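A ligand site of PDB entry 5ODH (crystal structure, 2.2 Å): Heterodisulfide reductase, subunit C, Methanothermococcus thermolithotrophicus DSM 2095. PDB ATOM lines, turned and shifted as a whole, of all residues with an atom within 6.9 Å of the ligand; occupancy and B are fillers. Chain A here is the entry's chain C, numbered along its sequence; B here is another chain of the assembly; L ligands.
The side-chain sulfur of Cys 37 binds an iron atom (FE2) of the ligand (2.5 Å).
FE1 of the ligand is bound by SG of Cys 87 (2.4 Å).
An iron atom (FE4) of the ligand is bound by the side-chain sulfur (SG) of Cys 40, 2.6 Å away.
An iron atom (FE3) of the ligand is bound by the side-chain sulfur of Cys 34, at 2.6 Å.
The backbone NH (N) of Cys 37 sits close to a sulfur (S1) of the ligand (3.7 Å).
The backbone NH (N) of Gly 38 lies close to a sulfur (S1) of the ligand, 3.7 Å away.
N of Tyr 35 touches S4 of the ligand, at 3.8 Å.
N of Gln 36 touches FE3 of the ligand (3.8 Å).
Val 91 touches the ligand.
Hydrophobic or aromatic side chains within 4 Å of the ligand: Tyr 35 and Val 91.
Within 4 Å of the ligand: Cys 34, Tyr 35, Gln 36, Cys 37, Gly 38, Cys 40, Cys 87 and Val 91.
The side-chain amide oxygen (OE1) of Gln 36 sits at hydrogen-bond distance from the guanidinium group (NH2) of Arg 55 (2.9 Å).
The side-chain sulfur (SG) of Cys 37 sits close to the side-chain hydroxyl (OG1) of Thr 39 (3.0 Å).
The side-chain sulfur (SG) of Cys 34 lies close to the side-chain amide nitrogen (NE2) of Gln 36 (3.0 Å).
SG of Cys 87 lies close to N of Val 91 (3.2 Å).
SG of Cys 87 lies close to N of Asp 90.
The side-chain sulfur (SG) of Cys 40 sits close to the backbone NH (N) of Arg 55, 3.4 Å away.
The backbone NH (N) of Arg 456 of chain B is in hydrogen-bond range of the backbone carbonyl oxygen (O) of Cys 37 (3.0 Å).
The side-chain sulfur (SG) of Cys 40 sits close to the side-chain hydroxyl (OG1) of Thr 41 (3.6 Å).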
ATOM      1  N   LEU A  31       1.943  -6.746  13.231  1.00  0.00           N
ATOM      2  CA  LEU A  31       0.957  -7.572  12.546  1.00  0.00           C
ATOM      3  C   LEU A  31       0.158  -8.432  13.517  1.00  0.00           C
ATOM      4  O   LEU A  31      -1.012  -8.724  13.268  1.00  0.00           O
ATOM      5  CB  LEU A  31       1.690  -8.473  11.535  1.00  0.00           C
ATOM      6  CG  LEU A  31       0.986  -9.719  10.968  1.00  0.00           C
ATOM      7  CD1 LEU A  31      -0.021  -9.299   9.932  1.00  0.00           C
ATOM      8  CD2 LEU A  31       1.985 -10.690  10.382  1.00  0.00           C
ATOM      9  N   ALA A  33      -0.917  -7.601  16.375  1.00  0.00           N
ATOM     10  CA  ALA A  33      -1.840  -6.797  17.159  1.00  0.00           C
ATOM     11  C   ALA A  33      -3.191  -6.584  16.482  1.00  0.00           C
ATOM     12  O   ALA A  33      -4.122  -6.103  17.118  1.00  0.00           O
ATOM     13  CB  ALA A  33      -1.237  -5.428  17.456  1.00  0.00           C
ATOM     14  N   CYS A  34      -3.306  -6.948  15.208  1.00  0.00           N
ATOM     15  CA  CYS A  34      -4.543  -6.707  14.472  1.00  0.00           C
ATOM     16  C   CYS A  34      -5.696  -7.465  15.122  1.00  0.00           C
ATOM     17  O   CYS A  34      -5.559  -8.639  15.466  1.00  0.00           O
ATOM     18  CB  CYS A  34      -4.344  -7.143  13.017  1.00  0.00           C
ATOM     19  SG  CYS A  34      -5.806  -7.774  12.194  1.00  0.00           S
ATOM     20  N   TYR A  35      -6.825  -6.769  15.299  1.00  0.00           N
ATOM     21  CA  TYR A  35      -8.036  -7.403  15.818  1.00  0.00           C
ATOM     22  C   TYR A  35      -9.203  -7.273  14.831  1.00  0.00           C
ATOM     23  O   TYR A  35     -10.372  -7.239  15.223  1.00  0.00           O
ATOM     24  CB  TYR A  35      -8.412  -6.861  17.210  1.00  0.00           C
ATOM     25  CG  TYR A  35      -8.648  -5.369  17.369  1.00  0.00           C
ATOM     26  CD1 TYR A  35      -8.653  -4.501  16.283  1.00  0.00           C
ATOM     27  CD2 TYR A  35      -8.853  -4.839  18.633  1.00  0.00           C
ATOM     28  CE1 TYR A  35      -8.864  -3.154  16.456  1.00  0.00           C
ATOM     29  CE2 TYR A  35      -9.073  -3.490  18.811  1.00  0.00           C
ATOM     30  CZ  TYR A  35      -9.072  -2.651  17.724  1.00  0.00           C
ATOM     31  OH  TYR A  35      -9.293  -1.299  17.919  1.00  0.00           O
ATOM     32  N   GLN A  36      -8.878  -7.195  13.540  1.00  0.00           N
ATOM     33  CA  GLN A  36      -9.831  -7.459  12.456  1.00  0.00           C
ATOM     34  C   GLN A  36     -11.026  -6.518  12.487  1.00  0.00           C
ATOM     35  O   GLN A  36     -12.156  -6.900  12.198  1.00  0.00           O
ATOM     36  CB  GLN A  36     -10.305  -8.913  12.509  1.00  0.00           C
ATOM     37  CG  GLN A  36      -9.270  -9.921  12.044  1.00  0.00           C
ATOM     38  CD  GLN A  36      -8.872  -9.718  10.587  1.00  0.00           C
ATOM     39  OE1 GLN A  36      -9.667  -9.947   9.671  1.00  0.00           O
ATOM     40  NE2 GLN A  36      -7.632  -9.310  10.372  1.00  0.00           N
ATOM     41  N   CYS A  37     -10.772  -5.253  12.819  1.00  0.00           N
ATOM     42  CA  CYS A  37     -11.851  -4.279  12.880  1.00  0.00           C
ATOM     43  C   CYS A  37     -12.330  -3.845  11.494  1.00  0.00           C
ATOM     44  O   CYS A  37     -13.512  -3.535  11.317  1.00  0.00           O
ATOM     45  CB  CYS A  37     -11.426  -3.082  13.715  1.00  0.00           C
ATOM     46  SG  CYS A  37     -10.572  -1.756  12.821  1.00  0.00           S
ATOM     47  N   GLY A  38     -11.437  -3.811  10.512  1.00  0.00           N
ATOM     48  CA  GLY A  38     -11.800  -3.415   9.162  1.00  0.00           C
ATOM     49  C   GLY A  38     -11.706  -1.923   8.866  1.00  0.00           C
ATOM     50  O   GLY A  38     -12.182  -1.498   7.805  1.00  0.00           O
ATOM     51  N   THR A  39     -11.129  -1.130   9.769  1.00  0.00           N
ATOM     52  CA  THR A  39     -10.924   0.301   9.488  1.00  0.00           C
ATOM     53  C   THR A  39     -10.010   0.492   8.277  1.00  0.00           C
ATOM     54  O   THR A  39     -10.207   1.428   7.490  1.00  0.00           O
ATOM     55  CB  THR A  39     -10.338   1.004  10.713  1.00  0.00           C
ATOM     56  OG1 THR A  39     -11.290   0.941  11.787  1.00  0.00           O
ATOM     57  CG2 THR A  39     -10.010   2.454  10.417  1.00  0.00           C
ATOM     58  N   CYS A  40      -9.003  -0.365   8.126  1.00  0.00           N
ATOM     59  CA  CYS A  40      -8.110  -0.253   6.991  1.00  0.00           C
ATOM     60  C   CYS A  40      -8.852  -0.454   5.676  1.00  0.00           C
ATOM     61  O   CYS A  40      -8.701   0.331   4.736  1.00  0.00           O
ATOM     62  CB  CYS A  40      -6.987  -1.284   7.114  1.00  0.00           C
ATOM     63  SG  CYS A  40      -7.607  -2.982   7.057  1.00  0.00           S
ATOM     64  N   THR A  41      -9.691  -1.493   5.609  1.00  0.00           N
ATOM     65  CA  THR A  41     -10.416  -1.791   4.382  1.00  0.00           C
ATOM     66  C   THR A  41     -11.336  -0.643   3.995  1.00  0.00           C
ATOM     67  O   THR A  41     -11.482  -0.344   2.799  1.00  0.00           O
ATOM     68  CB  THR A  41     -11.206  -3.080   4.560  1.00  0.00           C
ATOM     69  OG1 THR A  41     -10.332  -4.128   4.996  1.00  0.00           O
ATOM     70  CG2 THR A  41     -11.865  -3.486   3.239  1.00  0.00           C
ATOM     71  N   THR A  54      -7.942  -5.070   2.502  1.00  0.00           N
ATOM     72  CA  THR A  54      -6.731  -4.975   3.298  1.00  0.00           C
ATOM     73  C   THR A  54      -6.794  -5.888   4.509  1.00  0.00           C
ATOM     74  O   THR A  54      -5.847  -6.619   4.813  1.00  0.00           O
ATOM     75  CB  THR A  54      -6.520  -3.530   3.738  1.00  0.00           C
ATOM     76  OG1 THR A  54      -6.631  -2.664   2.606  1.00  0.00           O
ATOM     77  CG2 THR A  54      -5.139  -3.371   4.376  1.00  0.00           C
ATOM     78  N   ARG A  55      -7.923  -5.860   5.228  1.00  0.00           N
ATOM     79  CA  ARG A  55      -8.068  -6.656   6.435  1.00  0.00           C
ATOM     80  C   ARG A  55      -7.899  -8.147   6.134  1.00  0.00           C
ATOM     81  O   ARG A  55      -7.355  -8.889   6.953  1.00  0.00           O
ATOM     82  CB  ARG A  55      -9.435  -6.381   7.074  1.00  0.00           C
ATOM     83  CG  ARG A  55      -9.848  -7.354   8.178  1.00  0.00           C
ATOM     84  CD  ARG A  55     -11.281  -7.158   8.576  1.00  0.00           C
ATOM     85  NE  ARG A  55     -12.178  -7.530   7.485  1.00  0.00           N
ATOM     86  CZ  ARG A  55     -12.417  -8.774   7.110  1.00  0.00           C
ATOM     87  NH1 ARG A  55     -13.245  -9.027   6.101  1.00  0.00           N
ATOM     88  NH2 ARG A  55     -11.816  -9.790   7.732  1.00  0.00           N
ATOM     89  N   ILE A  58      -4.157  -9.200   6.052  1.00  0.00           N
ATOM     90  CA  ILE A  58      -3.669  -9.408   7.414  1.00  0.00           C
ATOM     91  C   ILE A  58      -4.235 -10.703   7.979  1.00  0.00           C
ATOM     92  O   ILE A  58      -3.507 -11.500   8.584  1.00  0.00           O
ATOM     93  CB  ILE A  58      -4.038  -8.202   8.300  1.00  0.00           C
ATOM     94  CG1 ILE A  58      -3.542  -6.885   7.684  1.00  0.00           C
ATOM     95  CG2 ILE A  58      -3.496  -8.395   9.712  1.00  0.00           C
ATOM     96  CD1 ILE A  58      -2.050  -6.775   7.553  1.00  0.00           C
ATOM     97  N   LEU A  62      -2.165 -14.091   9.426  1.00  0.00           N
ATOM     98  CA  LEU A  62      -2.277 -14.640  10.773  1.00  0.00           C
ATOM     99  C   LEU A  62      -2.727 -16.092  10.763  1.00  0.00           C
ATOM    100  O   LEU A  62      -2.294 -16.882  11.609  1.00  0.00           O
ATOM    101  CB  LEU A  62      -3.242 -13.796  11.594  1.00  0.00           C
ATOM    102  CG  LEU A  62      -2.757 -12.389  11.955  1.00  0.00           C
ATOM    103  CD1 LEU A  62      -3.940 -11.471  12.185  1.00  0.00           C
ATOM    104  CD2 LEU A  62      -1.879 -12.424  13.204  1.00  0.00           C
ATOM    105  N   CYS A  83      -4.381   3.573   6.015  1.00  0.00           N
ATOM    106  CA  CYS A  83      -4.707   2.616   7.060  1.00  0.00           C
ATOM    107  C   CYS A  83      -3.729   2.730   8.224  1.00  0.00           C
ATOM    108  O   CYS A  83      -4.134   2.701   9.394  1.00  0.00           O
ATOM    109  CB  CYS A  83      -4.669   1.195   6.494  1.00  0.00           C
ATOM    110  SG  CYS A  83      -2.990   0.741   6.067  1.00  0.00           S
ATOM    111  N   ARG A  86      -4.819   5.401  10.525  1.00  0.00           N
ATOM    112  CA  ARG A  86      -6.088   5.258  11.241  1.00  0.00           C
ATOM    113  C   ARG A  86      -6.214   3.983  12.051  1.00  0.00           C
ATOM    114  O   ARG A  86      -7.177   3.860  12.811  1.00  0.00           O
ATOM    115  CB  ARG A  86      -7.242   5.306  10.245  1.00  0.00           C
ATOM    116  CG  ARG A  86      -7.244   6.538   9.429  1.00  0.00           C
ATOM    117  CD  ARG A  86      -8.430   6.547   8.536  1.00  0.00           C
ATOM    118  NE  ARG A  86      -8.491   7.784   7.802  1.00  0.00           N
ATOM    119  CZ  ARG A  86      -9.176   7.952   6.686  1.00  0.00           C
ATOM    120  NH1 ARG A  86      -9.864   6.928   6.173  1.00  0.00           N
ATOM    121  NH2 ARG A  86      -9.174   9.126   6.068  1.00  0.00           N
ATOM    122  N   CYS A  87      -5.320   3.031  11.898  1.00  0.00           N
ATOM    123  CA  CYS A  87      -5.483   1.763  12.574  1.00  0.00           C
ATOM    124  C   CYS A  87      -5.466   1.986  14.079  1.00  0.00           C
ATOM    125  O   CYS A  87      -4.506   2.546  14.605  1.00  0.00           O
ATOM    126  CB  CYS A  87      -4.388   0.791  12.162  1.00  0.00           C
ATOM    127  SG  CYS A  87      -4.118  -0.476  13.391  1.00  0.00           S
ATOM    128  N   PRO A  88      -6.501   1.535  14.809  1.00  0.00           N
ATOM    129  CA  PRO A  88      -6.521   1.756  16.269  1.00  0.00           C
ATOM    130  C   PRO A  88      -5.555   0.867  17.024  1.00  0.00           C
ATOM    131  O   PRO A  88      -5.380   1.063  18.237  1.00  0.00           O
ATOM    132  CB  PRO A  88      -7.966   1.453  16.641  1.00  0.00           C
ATOM    133  CG  PRO A  88      -8.419   0.489  15.607  1.00  0.00           C
ATOM    134  CD  PRO A  88      -7.732   0.901  14.344  1.00  0.00           C
ATOM    135  N   ARG A  89      -4.936  -0.113  16.361  1.00  0.00           N
ATOM    136  CA  ARG A  89      -4.047  -1.051  17.016  1.00  0.00           C
ATOM    137  C   ARG A  89      -2.583  -0.843  16.650  1.00  0.00           C
ATOM    138  O   ARG A  89      -1.750  -1.720  16.949  1.00  0.00           O
ATOM    139  CB  ARG A  89      -4.496  -2.486  16.687  1.00  0.00           C
ATOM    140  CG  ARG A  89      -5.484  -3.059  17.693  1.00  0.00           C
ATOM    141  CD  ARG A  89      -4.785  -3.357  19.008  1.00  0.00           C
ATOM    142  NE  ARG A  89      -5.665  -3.982  19.998  1.00  0.00           N
ATOM    143  CZ  ARG A  89      -5.791  -5.288  20.167  1.00  0.00           C
ATOM    144  NH1 ARG A  89      -5.110  -6.140  19.402  1.00  0.00           N
ATOM    145  NH2 ARG A  89      -6.612  -5.762  21.103  1.00  0.00           N
ATOM    146  N   ASP A  90      -2.236   0.284  16.043  1.00  0.00           N
ATOM    147  CA  ASP A  90      -0.849   0.613  15.703  1.00  0.00           C
ATOM    148  C   ASP A  90      -0.235  -0.409  14.752  1.00  0.00           C
ATOM    149  O   ASP A  90       0.988  -0.607  14.751  1.00  0.00           O
ATOM    150  CB  ASP A  90       0.023   0.768  16.956  1.00  0.00           C
ATOM    151  CG  ASP A  90       0.078   2.193  17.477  1.00  0.00           C
ATOM    152  OD1 ASP A  90      -0.278   3.117  16.724  1.00  0.00           O
ATOM    153  OD2 ASP A  90       0.511   2.385  18.634  1.00  0.00           O
ATOM    154  N   VAL A  91      -1.065  -1.056  13.947  1.00  0.00           N
ATOM    155  CA  VAL A  91      -0.554  -1.980  12.942  1.00  0.00           C
ATOM    156  C   VAL A  91       0.120  -1.197  11.836  1.00  0.00           C
ATOM    157  O   VAL A  91      -0.470  -0.295  11.233  1.00  0.00           O
ATOM    158  CB  VAL A  91      -1.689  -2.863  12.386  1.00  0.00           C
ATOM    159  CG1 VAL A  91      -1.163  -3.800  11.308  1.00  0.00           C
ATOM    160  CG2 VAL A  91      -2.330  -3.654  13.514  1.00  0.00           C
ATOM    161  N   LYS A  92       1.381  -1.535  11.555  1.00  0.00           N
ATOM    162  CA  LYS A  92       2.162  -0.877  10.520  1.00  0.00           C
ATOM    163  C   LYS A  92       1.884  -1.570   9.177  1.00  0.00           C
ATOM    164  O   LYS A  92       2.727  -2.237   8.574  1.00  0.00           O
ATOM    165  CB  LYS A  92       3.648  -0.903  10.869  1.00  0.00           C
ATOM    166  CG  LYS A  92       3.987  -0.407  12.291  1.00  0.00           C
ATOM    167  CD  LYS A  92       4.069   1.106  12.367  1.00  0.00           C
ATOM    168  CE  LYS A  92       4.559   1.596  13.728  1.00  0.00           C
ATOM    169  NZ  LYS A  92       3.470   1.727  14.734  1.00  0.00           N
ATOM    170  N   VAL A  93       0.643  -1.389   8.710  1.00  0.00           N
ATOM    171  CA  VAL A  93       0.117  -2.182   7.605  1.00  0.00           C
ATOM    172  C   VAL A  93       0.969  -2.005   6.350  1.00  0.00           C
ATOM    173  O   VAL A  93       1.280  -2.968   5.648  1.00  0.00           O
ATOM    174  CB  VAL A  93      -1.356  -1.820   7.345  1.00  0.00           C
ATOM    175  CG1 VAL A  93      -1.917  -2.618   6.179  1.00  0.00           C
ATOM    176  CG2 VAL A  93      -2.203  -2.028   8.600  1.00  0.00           C
ATOM    177  N   MET B 428     -17.140  -3.564  16.866  1.00  0.00           N
ATOM    178  CA  MET B 428     -16.108  -4.586  16.738  1.00  0.00           C
ATOM    179  C   MET B 428     -16.441  -5.827  17.558  1.00  0.00           C
ATOM    180  O   MET B 428     -16.474  -6.933  17.022  1.00  0.00           O
ATOM    181  CB  MET B 428     -14.752  -4.041  17.188  1.00  0.00           C
ATOM    182  CG  MET B 428     -14.202  -2.936  16.306  1.00  0.00           C
ATOM    183  SD  MET B 428     -12.504  -2.591  16.756  1.00  0.00           S
ATOM    184  CE  MET B 428     -12.700  -2.000  18.434  1.00  0.00           C
ATOM    185  N   ARG B 456     -15.511  -1.413  12.149  1.00  0.00           N
ATOM    186  CA  ARG B 456     -15.186  -0.113  12.723  1.00  0.00           C
ATOM    187  C   ARG B 456     -15.088   0.926  11.613  1.00  0.00           C
ATOM    188  O   ARG B 456     -14.217   0.791  10.739  1.00  0.00           O
ATOM    189  CB  ARG B 456     -13.882  -0.191  13.497  1.00  0.00           C
ATOM    190  CG  ARG B 456     -13.521   1.068  14.258  1.00  0.00           C
ATOM    191  CD  ARG B 456     -12.167   0.937  14.910  1.00  0.00           C
ATOM    192  NE  ARG B 456     -11.752   2.167  15.569  1.00  0.00           N
ATOM    193  CZ  ARG B 456     -11.253   3.214  14.932  1.00  0.00           C
ATOM    194  NH1 ARG B 456     -11.088   3.199  13.617  1.00  0.00           N
ATOM    195  NH2 ARG B 456     -10.913   4.297  15.613  1.00  0.00           N
HETATM  196 FE1  LIG L   1      -5.385  -2.200  12.253  1.00  0.00          FE
HETATM  197 FE2  LIG L   1      -8.438  -2.973  12.280  1.00  0.00          FE
HETATM  198 FE3  LIG L   1      -6.194  -5.234  11.776  1.00  0.00          FE
HETATM  199 FE4  LIG L   1      -6.818  -3.027   9.515  1.00  0.00          FE
HETATM  200  S1  LIG L   1      -7.799  -4.319  10.820  1.00  0.00           S
HETATM  201  S2  LIG L   1      -5.279  -3.651  10.770  1.00  0.00           S
HETATM  202  S3  LIG L   1      -7.105  -1.808  11.176  1.00  0.00           S
HETATM  203  S4  LIG L   1      -6.639  -3.649  13.058  1.00  0.00           S
